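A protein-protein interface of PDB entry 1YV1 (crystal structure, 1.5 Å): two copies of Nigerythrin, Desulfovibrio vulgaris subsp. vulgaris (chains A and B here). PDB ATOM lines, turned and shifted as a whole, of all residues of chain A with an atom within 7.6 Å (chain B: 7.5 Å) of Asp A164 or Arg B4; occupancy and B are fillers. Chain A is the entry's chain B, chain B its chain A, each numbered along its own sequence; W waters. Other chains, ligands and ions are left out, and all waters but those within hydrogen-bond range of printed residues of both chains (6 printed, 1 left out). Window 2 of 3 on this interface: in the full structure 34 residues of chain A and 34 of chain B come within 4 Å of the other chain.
Ala A159 touches none of the printed residues of chain B. Of the printed residues of chain B, Tyr A160 touches Asn B15 (3.0 Å). Of chain B, only Arg B4 (3.9 Å), Ala B13 (3.2 Å) and Thr B14 (2.6 Å) come within 4 Å of Asp A164. Printed residues of chain B within 4 Å of Asp A167: Lys B2 (3.0 Å). Printed residues of chain A within 4 Å of Met B1: Asn A161 (3.8 Å) and Asp A162 (3.2 Å). Of chain A, only Asp A164 (3.9 Å) comes within 4 Å of Arg B4. Leu B147 touches none of the printed residues of chain A. The nearest residue of chain B that does not touch Asp A164 is Asn B12 (4.2 Å). The nearest printed residue of chain A that does not touch Thr B14 is Tyr A160 (6.4 Å).
Hydrophobic or aromatic side chains of chain A within 4 Å of the printed part of chain B: Tyr A59, Tyr A160 and Ile A163.
The guanidinium group (NE) of Arg B4 lies close to the side-chain amide nitrogen (NE2) of Gln B6 (3.4 Å). NH1 of Arg B4 is in hydrogen-bond range of OD1 of Asn B12 (3.1 Å).
CG of Met B1 touches O of Asn A161, at 3.8 Å. Asp A162 touches Met B1. Ile A163 touches Thr B14. CG2 of Ile A163 touches CB of Asn B15, 3.7 Å away. OD2 of Asp A164 touches CA of Ala B13 (3.2 Å). Pro A166 touches Lys B2 (O to NZ, 3.6 Å).
N of Lys B2 sits at hydrogen-bond distance from OD1 of Asp A162 (2.6 Å). The side-chain amino group (NZ) of Lys B2 sits at hydrogen-bond distance from the backbone carbonyl oxygen (O) of Ala A165. The side-chain carboxylate (OD2) of Asp A167 is in salt-bridge range of the side-chain amino group (NZ) of Lys B2 (3.0 Å). The side-chain carboxylate (OD2) of Asp A164 is in salt-bridge range of the guanidinium group (NH1) of Arg B4. The side-chain hydroxyl (OG1) of Thr B14 lies within hydrogen-bond range of the side-chain hydroxyl (OH) of Tyr A59 (2.7 Å). The side-chain carboxylate (OD1) of Asp A164 is in hydrogen-bond range of the side-chain hydroxyl (OG1) of Thr B14. The backbone carbonyl oxygen (O) of Tyr A160 lies within hydrogen-bond range of the side-chain amide nitrogen (ND2) of Asn B15 (3.0 Å).
Water W2 lies within hydrogen-bond range of OH of Tyr A160 (2.6 Å) and O of Asn B15 (3.5 Å). Water W3 bridges OD2 of Asp A164 (2.7 Å) and NH1 of Arg B4 (2.7 Å). Water W6 bridges the side-chain carboxylate (OD2) of Asp A162 (2.8 Å) and the backbone NH (N) of Met B1 (3.0 Å). Water W5 lies within hydrogen-bond range of the backbone carbonyl oxygen (O) of Thr B14 (2.8 Å) and the side-chain hydroxyl (OH) of Tyr A59 (3.0 Å). Water W1 lies within hydrogen-bond range of O of Asn A161 (2.8 Å) and ND2 of Asn B15 (3.0 Å). Water W4 lies within hydrogen-bond range of OD2 of Asp A162 (3.0 Å) and N of Met B1 (3.1 Å).
No position is printed for both chains.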
ATOM      1  N   TYR A  59      18.320 -15.223  -9.890  1.00  0.00           N
ATOM      2  CA  TYR A  59      16.887 -15.046 -10.122  1.00  0.00           C
ATOM      3  C   TYR A  59      16.190 -16.401 -10.003  1.00  0.00           C
ATOM      4  O   TYR A  59      15.824 -17.014 -11.005  1.00  0.00           O
ATOM      5  CB  TYR A  59      16.629 -14.469 -11.516  1.00  0.00           C
ATOM      6  CG  TYR A  59      17.264 -13.122 -11.786  1.00  0.00           C
ATOM      7  CD1 TYR A  59      18.443 -13.021 -12.525  1.00  0.00           C
ATOM      8  CD2 TYR A  59      16.650 -11.945 -11.361  1.00  0.00           C
ATOM      9  CE1 TYR A  59      18.987 -11.777 -12.846  1.00  0.00           C
ATOM     10  CE2 TYR A  59      17.188 -10.697 -11.673  1.00  0.00           C
ATOM     11  CZ  TYR A  59      18.352 -10.620 -12.421  1.00  0.00           C
ATOM     12  OH  TYR A  59      18.863  -9.389 -12.769  1.00  0.00           O
ATOM     13  N   ILE A  62      12.487 -16.502 -11.524  1.00  0.00           N
ATOM     14  CA  ILE A  62      12.491 -16.476 -12.979  1.00  0.00           C
ATOM     15  C   ILE A  62      13.003 -17.815 -13.511  1.00  0.00           C
ATOM     16  O   ILE A  62      12.523 -18.308 -14.532  1.00  0.00           O
ATOM     17  CB  ILE A  62      13.352 -15.302 -13.516  1.00  0.00           C
ATOM     18  CG1 ILE A  62      12.613 -13.981 -13.265  1.00  0.00           C
ATOM     19  CG2 ILE A  62      13.625 -15.486 -15.007  1.00  0.00           C
ATOM     20  CD1 ILE A  62      13.428 -12.741 -13.583  1.00  0.00           C
ATOM     21  N   ALA A 159       7.410 -10.961 -15.687  1.00  0.00           N
ATOM     22  CA  ALA A 159       8.632 -11.220 -14.937  1.00  0.00           C
ATOM     23  C   ALA A 159       9.698 -10.174 -15.247  1.00  0.00           C
ATOM     24  O   ALA A 159      10.487  -9.810 -14.382  1.00  0.00           O
ATOM     25  CB  ALA A 159       9.153 -12.610 -15.256  1.00  0.00           C
ATOM     26  N   TYR A 160       9.716  -9.699 -16.489  1.00  0.00           N
ATOM     27  CA  TYR A 160      10.668  -8.682 -16.926  1.00  0.00           C
ATOM     28  C   TYR A 160      10.392  -7.372 -16.184  1.00  0.00           C
ATOM     29  O   TYR A 160      11.306  -6.730 -15.662  1.00  0.00           O
ATOM     30  CB  TYR A 160      10.516  -8.465 -18.433  1.00  0.00           C
ATOM     31  CG  TYR A 160      11.436  -7.426 -19.041  1.00  0.00           C
ATOM     32  CD1 TYR A 160      12.729  -7.757 -19.451  1.00  0.00           C
ATOM     33  CD2 TYR A 160      10.991  -6.123 -19.260  1.00  0.00           C
ATOM     34  CE1 TYR A 160      13.551  -6.811 -20.075  1.00  0.00           C
ATOM     35  CE2 TYR A 160      11.801  -5.176 -19.877  1.00  0.00           C
ATOM     36  CZ  TYR A 160      13.078  -5.522 -20.285  1.00  0.00           C
ATOM     37  OH  TYR A 160      13.876  -4.583 -20.905  1.00  0.00           O
ATOM     38  N   ASN A 161       9.122  -6.983 -16.133  1.00  0.00           N
ATOM     39  CA  ASN A 161       8.739  -5.748 -15.458  1.00  0.00           C
ATOM     40  C   ASN A 161       9.017  -5.788 -13.967  1.00  0.00           C
ATOM     41  O   ASN A 161       9.296  -4.756 -13.363  1.00  0.00           O
ATOM     42  CB  ASN A 161       7.258  -5.447 -15.698  1.00  0.00           C
ATOM     43  CG  ASN A 161       6.989  -5.034 -17.119  1.00  0.00           C
ATOM     44  OD1 ASN A 161       7.865  -4.477 -17.773  1.00  0.00           O
ATOM     45  ND2 ASN A 161       5.782  -5.287 -17.606  1.00  0.00           N
ATOM     46  N   ASP A 162       8.937  -6.981 -13.384  1.00  0.00           N
ATOM     47  CA  ASP A 162       9.187  -7.166 -11.954  1.00  0.00           C
ATOM     48  C   ASP A 162      10.488  -7.925 -11.714  1.00  0.00           C
ATOM     49  O   ASP A 162      10.631  -8.623 -10.712  1.00  0.00           O
ATOM     50  CB  ASP A 162       8.037  -7.947 -11.306  1.00  0.00           C
ATOM     51  CG  ASP A 162       6.737  -7.180 -11.306  1.00  0.00           C
ATOM     52  OD1 ASP A 162       6.782  -5.946 -11.119  1.00  0.00           O
ATOM     53  OD2 ASP A 162       5.669  -7.812 -11.472  1.00  0.00           O
ATOM     54  N   ILE A 163      11.451  -7.771 -12.614  1.00  0.00           N
ATOM     55  CA  ILE A 163      12.708  -8.494 -12.482  1.00  0.00           C
ATOM     56  C   ILE A 163      13.415  -8.276 -11.141  1.00  0.00           C
ATOM     57  O   ILE A 163      14.111  -9.168 -10.655  1.00  0.00           O
ATOM     58  CB  ILE A 163      13.666  -8.139 -13.641  1.00  0.00           C
ATOM     59  CG1 ILE A 163      14.827  -9.134 -13.682  1.00  0.00           C
ATOM     60  CG2 ILE A 163      14.181  -6.713 -13.480  1.00  0.00           C
ATOM     61  CD1 ILE A 163      15.649  -9.061 -14.957  1.00  0.00           C
ATOM     62  N   ASP A 164      13.224  -7.106 -10.537  1.00  0.00           N
ATOM     63  CA  ASP A 164      13.860  -6.802  -9.258  1.00  0.00           C
ATOM     64  C   ASP A 164      12.879  -6.834  -8.098  1.00  0.00           C
ATOM     65  O   ASP A 164      13.169  -6.337  -7.005  1.00  0.00           O
ATOM     66  CB  ASP A 164      14.545  -5.440  -9.336  1.00  0.00           C
ATOM     67  CG  ASP A 164      15.577  -5.388 -10.438  1.00  0.00           C
ATOM     68  OD1 ASP A 164      16.458  -6.271 -10.443  1.00  0.00           O
ATOM     69  OD2 ASP A 164      15.503  -4.480 -11.298  1.00  0.00           O
ATOM     70  N   ALA A 165      11.715  -7.428  -8.343  1.00  0.00           N
ATOM     71  CA  ALA A 165      10.674  -7.552  -7.330  1.00  0.00           C
ATOM     72  C   ALA A 165      10.074  -8.956  -7.354  1.00  0.00           C
ATOM     73  O   ALA A 165       8.868  -9.130  -7.536  1.00  0.00           O
ATOM     74  CB  ALA A 165       9.582  -6.514  -7.568  1.00  0.00           C
ATOM     75  N   PRO A 166      10.914  -9.985  -7.179  1.00  0.00           N
ATOM     76  CA  PRO A 166      10.396 -11.354  -7.189  1.00  0.00           C
ATOM     77  C   PRO A 166       9.621 -11.638  -5.904  1.00  0.00           C
ATOM     78  O   PRO A 166       9.693 -10.871  -4.948  1.00  0.00           O
ATOM     79  CB  PRO A 166      11.663 -12.192  -7.292  1.00  0.00           C
ATOM     80  CG  PRO A 166      12.642 -11.386  -6.477  1.00  0.00           C
ATOM     81  CD  PRO A 166      12.372  -9.969  -6.960  1.00  0.00           C
ATOM     82  N   ASP A 167       8.861 -12.725  -5.897  1.00  0.00           N
ATOM     83  CA  ASP A 167       8.115 -13.115  -4.705  1.00  0.00           C
ATOM     84  C   ASP A 167       8.189 -14.631  -4.569  1.00  0.00           C
ATOM     85  O   ASP A 167       8.896 -15.284  -5.334  1.00  0.00           O
ATOM     86  CB  ASP A 167       6.660 -12.625  -4.768  1.00  0.00           C
ATOM     87  CG  ASP A 167       5.961 -13.008  -6.054  1.00  0.00           C
ATOM     88  OD1 ASP A 167       5.882 -14.214  -6.358  1.00  0.00           O
ATOM     89  OD2 ASP A 167       5.478 -12.096  -6.759  1.00  0.00           O
ATOM     90  N   MET B   1       3.126  -4.377 -12.811  1.00  0.00           N
ATOM     91  CA  MET B   1       4.439  -3.994 -12.218  1.00  0.00           C
ATOM     92  C   MET B   1       4.304  -3.680 -10.735  1.00  0.00           C
ATOM     93  O   MET B   1       3.508  -2.827 -10.335  1.00  0.00           O
ATOM     94  CB  MET B   1       5.011  -2.778 -12.940  1.00  0.00           C
ATOM     95  CG  MET B   1       6.436  -2.451 -12.535  1.00  0.00           C
ATOM     96  SD  MET B   1       7.011  -0.965 -13.344  1.00  0.00           S
ATOM     97  CE  MET B   1       8.477  -0.604 -12.396  1.00  0.00           C
ATOM     98  N   LYS B   2       5.104  -4.366  -9.927  1.00  0.00           N
ATOM     99  CA  LYS B   2       5.084  -4.195  -8.484  1.00  0.00           C
ATOM    100  C   LYS B   2       5.824  -2.945  -8.021  1.00  0.00           C
ATOM    101  O   LYS B   2       6.765  -2.481  -8.669  1.00  0.00           O
ATOM    102  CB  LYS B   2       5.690  -5.437  -7.822  1.00  0.00           C
ATOM    103  CG  LYS B   2       4.930  -6.714  -8.156  1.00  0.00           C
ATOM    104  CD  LYS B   2       5.716  -7.974  -7.813  1.00  0.00           C
ATOM    105  CE  LYS B   2       5.969  -8.106  -6.324  1.00  0.00           C
ATOM    106  NZ  LYS B   2       6.638  -9.403  -6.014  1.00  0.00           N
ATOM    107  N   VAL B   3       5.378  -2.403  -6.893  1.00  0.00           N
ATOM    108  CA  VAL B   3       5.986  -1.216  -6.309  1.00  0.00           C
ATOM    109  C   VAL B   3       7.173  -1.636  -5.448  1.00  0.00           C
ATOM    110  O   VAL B   3       7.015  -2.410  -4.503  1.00  0.00           O
ATOM    111  CB  VAL B   3       4.981  -0.457  -5.415  1.00  0.00           C
ATOM    112  CG1 VAL B   3       5.655   0.750  -4.782  1.00  0.00           C
ATOM    113  CG2 VAL B   3       3.777  -0.021  -6.236  1.00  0.00           C
ATOM    114  N   ARG B   4       8.356  -1.131  -5.786  1.00  0.00           N
ATOM    115  CA  ARG B   4       9.576  -1.434  -5.046  1.00  0.00           C
ATOM    116  C   ARG B   4       9.729  -0.413  -3.922  1.00  0.00           C
ATOM    117  O   ARG B   4       8.979   0.563  -3.859  1.00  0.00           O
ATOM    118  CB  ARG B   4      10.798  -1.364  -5.973  1.00  0.00           C
ATOM    119  CG  ARG B   4      10.822  -2.400  -7.098  1.00  0.00           C
ATOM    120  CD  ARG B   4      11.981  -2.135  -8.064  1.00  0.00           C
ATOM    121  NE  ARG B   4      13.281  -2.200  -7.398  1.00  0.00           N
ATOM    122  CZ  ARG B   4      14.428  -1.808  -7.944  1.00  0.00           C
ATOM    123  NH1 ARG B   4      14.449  -1.315  -9.176  1.00  0.00           N
ATOM    124  NH2 ARG B   4      15.559  -1.900  -7.251  1.00  0.00           N
ATOM    125  N   ALA B   5      10.698  -0.638  -3.040  1.00  0.00           N
ATOM    126  CA  ALA B   5      10.943   0.273  -1.926  1.00  0.00           C
ATOM    127  C   ALA B   5      11.506   1.588  -2.450  1.00  0.00           C
ATOM    128  O   ALA B   5      11.415   2.625  -1.792  1.00  0.00           O
ATOM    129  CB  ALA B   5      11.920  -0.355  -0.939  1.00  0.00           C
ATOM    130  N   GLN B   6      12.092   1.538  -3.640  1.00  0.00           N
ATOM    131  CA  GLN B   6      12.662   2.728  -4.251  1.00  0.00           C
ATOM    132  C   GLN B   6      12.253   2.849  -5.712  1.00  0.00           C
ATOM    133  O   GLN B   6      11.851   1.869  -6.342  1.00  0.00           O
ATOM    134  CB  GLN B   6      14.189   2.701  -4.157  1.00  0.00           C
ATOM    135  CG  GLN B   6      14.833   1.466  -4.768  1.00  0.00           C
ATOM    136  CD  GLN B   6      14.699   0.245  -3.882  1.00  0.00           C
ATOM    137  OE1 GLN B   6      15.174   0.232  -2.745  1.00  0.00           O
ATOM    138  NE2 GLN B   6      14.050  -0.793  -4.399  1.00  0.00           N
ATOM    139  N   VAL B   7      12.351   4.061  -6.244  1.00  0.00           N
ATOM    140  CA  VAL B   7      12.004   4.322  -7.634  1.00  0.00           C
ATOM    141  C   VAL B   7      13.034   3.651  -8.538  1.00  0.00           C
ATOM    142  O   VAL B   7      14.239   3.829  -8.357  1.00  0.00           O
ATOM    143  CB  VAL B   7      11.986   5.840  -7.921  1.00  0.00           C
ATOM    144  CG1 VAL B   7      11.643   6.092  -9.376  1.00  0.00           C
ATOM    145  CG2 VAL B   7      10.981   6.527  -7.013  1.00  0.00           C
ATOM    146  N   PRO B   8      12.573   2.862  -9.521  1.00  0.00           N
ATOM    147  CA  PRO B   8      13.492   2.178 -10.435  1.00  0.00           C
ATOM    148  C   PRO B   8      14.295   3.136 -11.314  1.00  0.00           C
ATOM    149  O   PRO B   8      13.762   4.109 -11.851  1.00  0.00           O
ATOM    150  CB  PRO B   8      12.563   1.267 -11.240  1.00  0.00           C
ATOM    151  CG  PRO B   8      11.273   2.026 -11.253  1.00  0.00           C
ATOM    152  CD  PRO B   8      11.171   2.528  -9.833  1.00  0.00           C
ATOM    153  N   THR B   9      15.586   2.852 -11.441  1.00  0.00           N
ATOM    154  CA  THR B   9      16.492   3.664 -12.245  1.00  0.00           C
ATOM    155  C   THR B   9      17.491   2.733 -12.915  1.00  0.00           C
ATOM    156  O   THR B   9      17.575   1.552 -12.578  1.00  0.00           O
ATOM    157  CB  THR B   9      17.294   4.651 -11.376  1.00  0.00           C
ATOM    158  OG1 THR B   9      18.164   3.913 -10.510  1.00  0.00           O
ATOM    159  CG2 THR B   9      16.363   5.517 -10.538  1.00  0.00           C
ATOM    160  N   LYS B  11      20.426   2.745 -12.443  1.00  0.00           N
ATOM    161  CA  LYS B  11      21.410   2.430 -11.413  1.00  0.00           C
ATOM    162  C   LYS B  11      21.012   1.264 -10.508  1.00  0.00           C
ATOM    163  O   LYS B  11      21.860   0.454 -10.140  1.00  0.00           O
ATOM    164  CB  LYS B  11      21.679   3.670 -10.554  1.00  0.00           C
ATOM    165  CG  LYS B  11      22.763   3.484  -9.508  1.00  0.00           C
ATOM    166  CD  LYS B  11      22.972   4.768  -8.719  1.00  0.00           C
ATOM    167  CE  LYS B  11      24.139   4.649  -7.751  1.00  0.00           C
ATOM    168  NZ  LYS B  11      25.425   4.412  -8.468  1.00  0.00           N
ATOM    169  N   ASN B  12      19.730   1.162 -10.157  1.00  0.00           N
ATOM    170  CA  ASN B  12      19.288   0.094  -9.258  1.00  0.00           C
ATOM    171  C   ASN B  12      18.453  -1.029  -9.875  1.00  0.00           C
ATOM    172  O   ASN B  12      18.020  -1.937  -9.160  1.00  0.00           O
ATOM    173  CB  ASN B  12      18.501   0.686  -8.084  1.00  0.00           C
ATOM    174  CG  ASN B  12      17.174   1.289  -8.512  1.00  0.00           C
ATOM    175  OD1 ASN B  12      16.573   0.862  -9.498  1.00  0.00           O
ATOM    176  ND2 ASN B  12      16.702   2.275  -7.759  1.00  0.00           N
ATOM    177  N   ALA B  13      18.222  -0.974 -11.183  1.00  0.00           N
ATOM    178  CA  ALA B  13      17.416  -1.994 -11.855  1.00  0.00           C
ATOM    179  C   ALA B  13      18.265  -2.908 -12.726  1.00  0.00           C
ATOM    180  O   ALA B  13      19.356  -2.535 -13.146  1.00  0.00           O
ATOM    181  CB  ALA B  13      16.342  -1.327 -12.700  1.00  0.00           C
ATOM    182  N   THR B  14      17.758  -4.103 -13.014  1.00  0.00           N
ATOM    183  CA  THR B  14      18.520  -5.039 -13.825  1.00  0.00           C
ATOM    184  C   THR B  14      17.886  -5.425 -15.158  1.00  0.00           C
ATOM    185  O   THR B  14      18.231  -6.452 -15.739  1.00  0.00           O
ATOM    186  CB  THR B  14      18.868  -6.314 -13.022  1.00  0.00           C
ATOM    187  OG1 THR B  14      17.671  -7.003 -12.638  1.00  0.00           O
ATOM    188  CG2 THR B  14      19.657  -5.935 -11.767  1.00  0.00           C
ATOM    189  N   ASN B  15      16.958  -4.603 -15.643  1.00  0.00           N
ATOM    190  CA  ASN B  15      16.347  -4.869 -16.940  1.00  0.00           C
ATOM    191  C   ASN B  15      16.613  -3.702 -17.889  1.00  0.00           C
ATOM    192  O   ASN B  15      15.742  -3.290 -18.656  1.00  0.00           O
ATOM    193  CB  ASN B  15      14.836  -5.153 -16.815  1.00  0.00           C
ATOM    194  CG  ASN B  15      14.061  -4.026 -16.155  1.00  0.00           C
ATOM    195  OD1 ASN B  15      14.630  -3.059 -15.653  1.00  0.00           O
ATOM    196  ND2 ASN B  15      12.736  -4.158 -16.149  1.00  0.00           N
ATOM    197  N   PHE B  16      17.834  -3.174 -17.819  1.00  0.00           N
ATOM    198  CA  PHE B  16      18.240  -2.067 -18.675  1.00  0.00           C
ATOM    199  C   PHE B  16      19.296  -2.458 -19.702  1.00  0.00           C
ATOM    200  O   PHE B  16      19.908  -1.596 -20.326  1.00  0.00           O
ATOM    201  CB  PHE B  16      18.751  -0.886 -17.841  1.00  0.00           C
ATOM    202  CG  PHE B  16      17.655  -0.029 -17.269  1.00  0.00           C
ATOM    203  CD1 PHE B  16      16.859  -0.494 -16.227  1.00  0.00           C
ATOM    204  CD2 PHE B  16      17.407   1.237 -17.787  1.00  0.00           C
ATOM    205  CE1 PHE B  16      15.830   0.289 -15.706  1.00  0.00           C
ATOM    206  CE2 PHE B  16      16.377   2.031 -17.275  1.00  0.00           C
ATOM    207  CZ  PHE B  16      15.588   1.551 -16.231  1.00  0.00           C
ATOM    208  N   LEU B 147      10.713   2.378 -19.005  1.00  0.00           N
ATOM    209  CA  LEU B 147       9.967   1.615 -18.012  1.00  0.00           C
ATOM    210  C   LEU B 147       8.485   1.524 -18.352  1.00  0.00           C
ATOM    211  O   LEU B 147       7.848   0.487 -18.141  1.00  0.00           O
ATOM    212  CB  LEU B 147      10.151   2.242 -16.626  1.00  0.00           C
ATOM    213  CG  LEU B 147      11.568   2.104 -16.065  1.00  0.00           C
ATOM    214  CD1 LEU B 147      11.743   3.007 -14.849  1.00  0.00           C
ATOM    215  CD2 LEU B 147      11.824   0.649 -15.705  1.00  0.00           C
ATOM    216  N   LYS B 188      -0.200   3.778  -5.829  1.00  0.00           N
ATOM    217  CA  LYS B 188       0.666   4.731  -6.505  1.00  0.00           C
ATOM    218  C   LYS B 188       1.376   4.113  -7.701  1.00  0.00           C
ATOM    219  O   LYS B 188       1.367   2.896  -7.890  1.00  0.00           O
ATOM    220  CB  LYS B 188       1.707   5.284  -5.529  1.00  0.00           C
ATOM    221  CG  LYS B 188       2.707   4.253  -5.032  1.00  0.00           C
ATOM    222  CD  LYS B 188       3.726   4.887  -4.095  1.00  0.00           C
ATOM    223  CE  LYS B 188       4.732   3.864  -3.590  1.00  0.00           C
ATOM    224  NZ  LYS B 188       5.704   4.456  -2.624  1.00  0.00           N
ATOM    225  N   CYS B 189       1.985   4.970  -8.510  1.00  0.00           N
ATOM    226  CA  CYS B 189       2.720   4.538  -9.690  1.00  0.00           C
ATOM    227  C   CYS B 189       4.015   3.837  -9.268  1.00  0.00           C
ATOM    228  O   CYS B 189       4.798   4.380  -8.489  1.00  0.00           O
ATOM    229  CB  CYS B 189       3.047   5.749 -10.558  1.00  0.00           C
ATOM    230  SG  CYS B 189       3.989   5.347 -12.033  1.00  0.00           S
ATOM    231  N   PRO B 190       4.254   2.616  -9.772  1.00  0.00           N
ATOM    232  CA  PRO B 190       5.474   1.886  -9.415  1.00  0.00           C
ATOM    233  C   PRO B 190       6.725   2.435 -10.093  1.00  0.00           C
ATOM    234  O   PRO B 190       7.846   2.103  -9.707  1.00  0.00           O
ATOM    235  CB  PRO B 190       5.157   0.460  -9.850  1.00  0.00           C
ATOM    236  CG  PRO B 190       4.313   0.679 -11.065  1.00  0.00           C
ATOM    237  CD  PRO B 190       3.377   1.789 -10.621  1.00  0.00           C
ATOM    238  N   ILE B 191       6.531   3.279 -11.101  1.00  0.00           N
ATOM    239  CA  ILE B 191       7.653   3.863 -11.820  1.00  0.00           C
ATOM    240  C   ILE B 191       8.127   5.183 -11.213  1.00  0.00           C
ATOM    241  O   ILE B 191       9.329   5.390 -11.056  1.00  0.00           O
ATOM    242  CB  ILE B 191       7.302   4.084 -13.316  1.00  0.00           C
ATOM    243  CG1 ILE B 191       7.121   2.726 -14.004  1.00  0.00           C
ATOM    244  CG2 ILE B 191       8.399   4.898 -14.005  1.00  0.00           C
ATOM    245  CD1 ILE B 191       6.682   2.816 -15.448  1.00  0.00           C
ATOM    246  N   PHE B 193       6.155   6.754  -8.406  1.00  0.00           N
ATOM    247  CA  PHE B 193       5.497   6.907  -7.105  1.00  0.00           C
ATOM    248  C   PHE B 193       4.354   7.919  -7.044  1.00  0.00           C
ATOM    249  O   PHE B 193       3.874   8.263  -5.961  1.00  0.00           O
ATOM    250  CB  PHE B 193       6.537   7.239  -6.025  1.00  0.00           C
ATOM    251  CG  PHE B 193       7.390   6.065  -5.617  1.00  0.00           C
ATOM    252  CD1 PHE B 193       7.341   4.864  -6.321  1.00  0.00           C
ATOM    253  CD2 PHE B 193       8.248   6.164  -4.527  1.00  0.00           C
ATOM    254  CE1 PHE B 193       8.133   3.781  -5.944  1.00  0.00           C
ATOM    255  CE2 PHE B 193       9.044   5.088  -4.142  1.00  0.00           C
ATOM    256  CZ  PHE B 193       8.987   3.895  -4.851  1.00  0.00           C
HETATM  257  O   HOH W   1      10.546  -2.675 -14.746  1.00  0.00           O
HETATM  258  O   HOH W   2      16.350  -5.397 -21.345  1.00  0.00           O
HETATM  259  O   HOH W   3      13.427  -2.821 -11.234  1.00  0.00           O
HETATM  260  O   HOH W   4       4.500  -6.826 -14.011  1.00  0.00           O
HETATM  261  O   HOH W   5      19.180  -9.063 -15.765  1.00  0.00           O
HETATM  262  O   HOH W   6       3.020  -6.984 -11.374  1.00  0.00           O
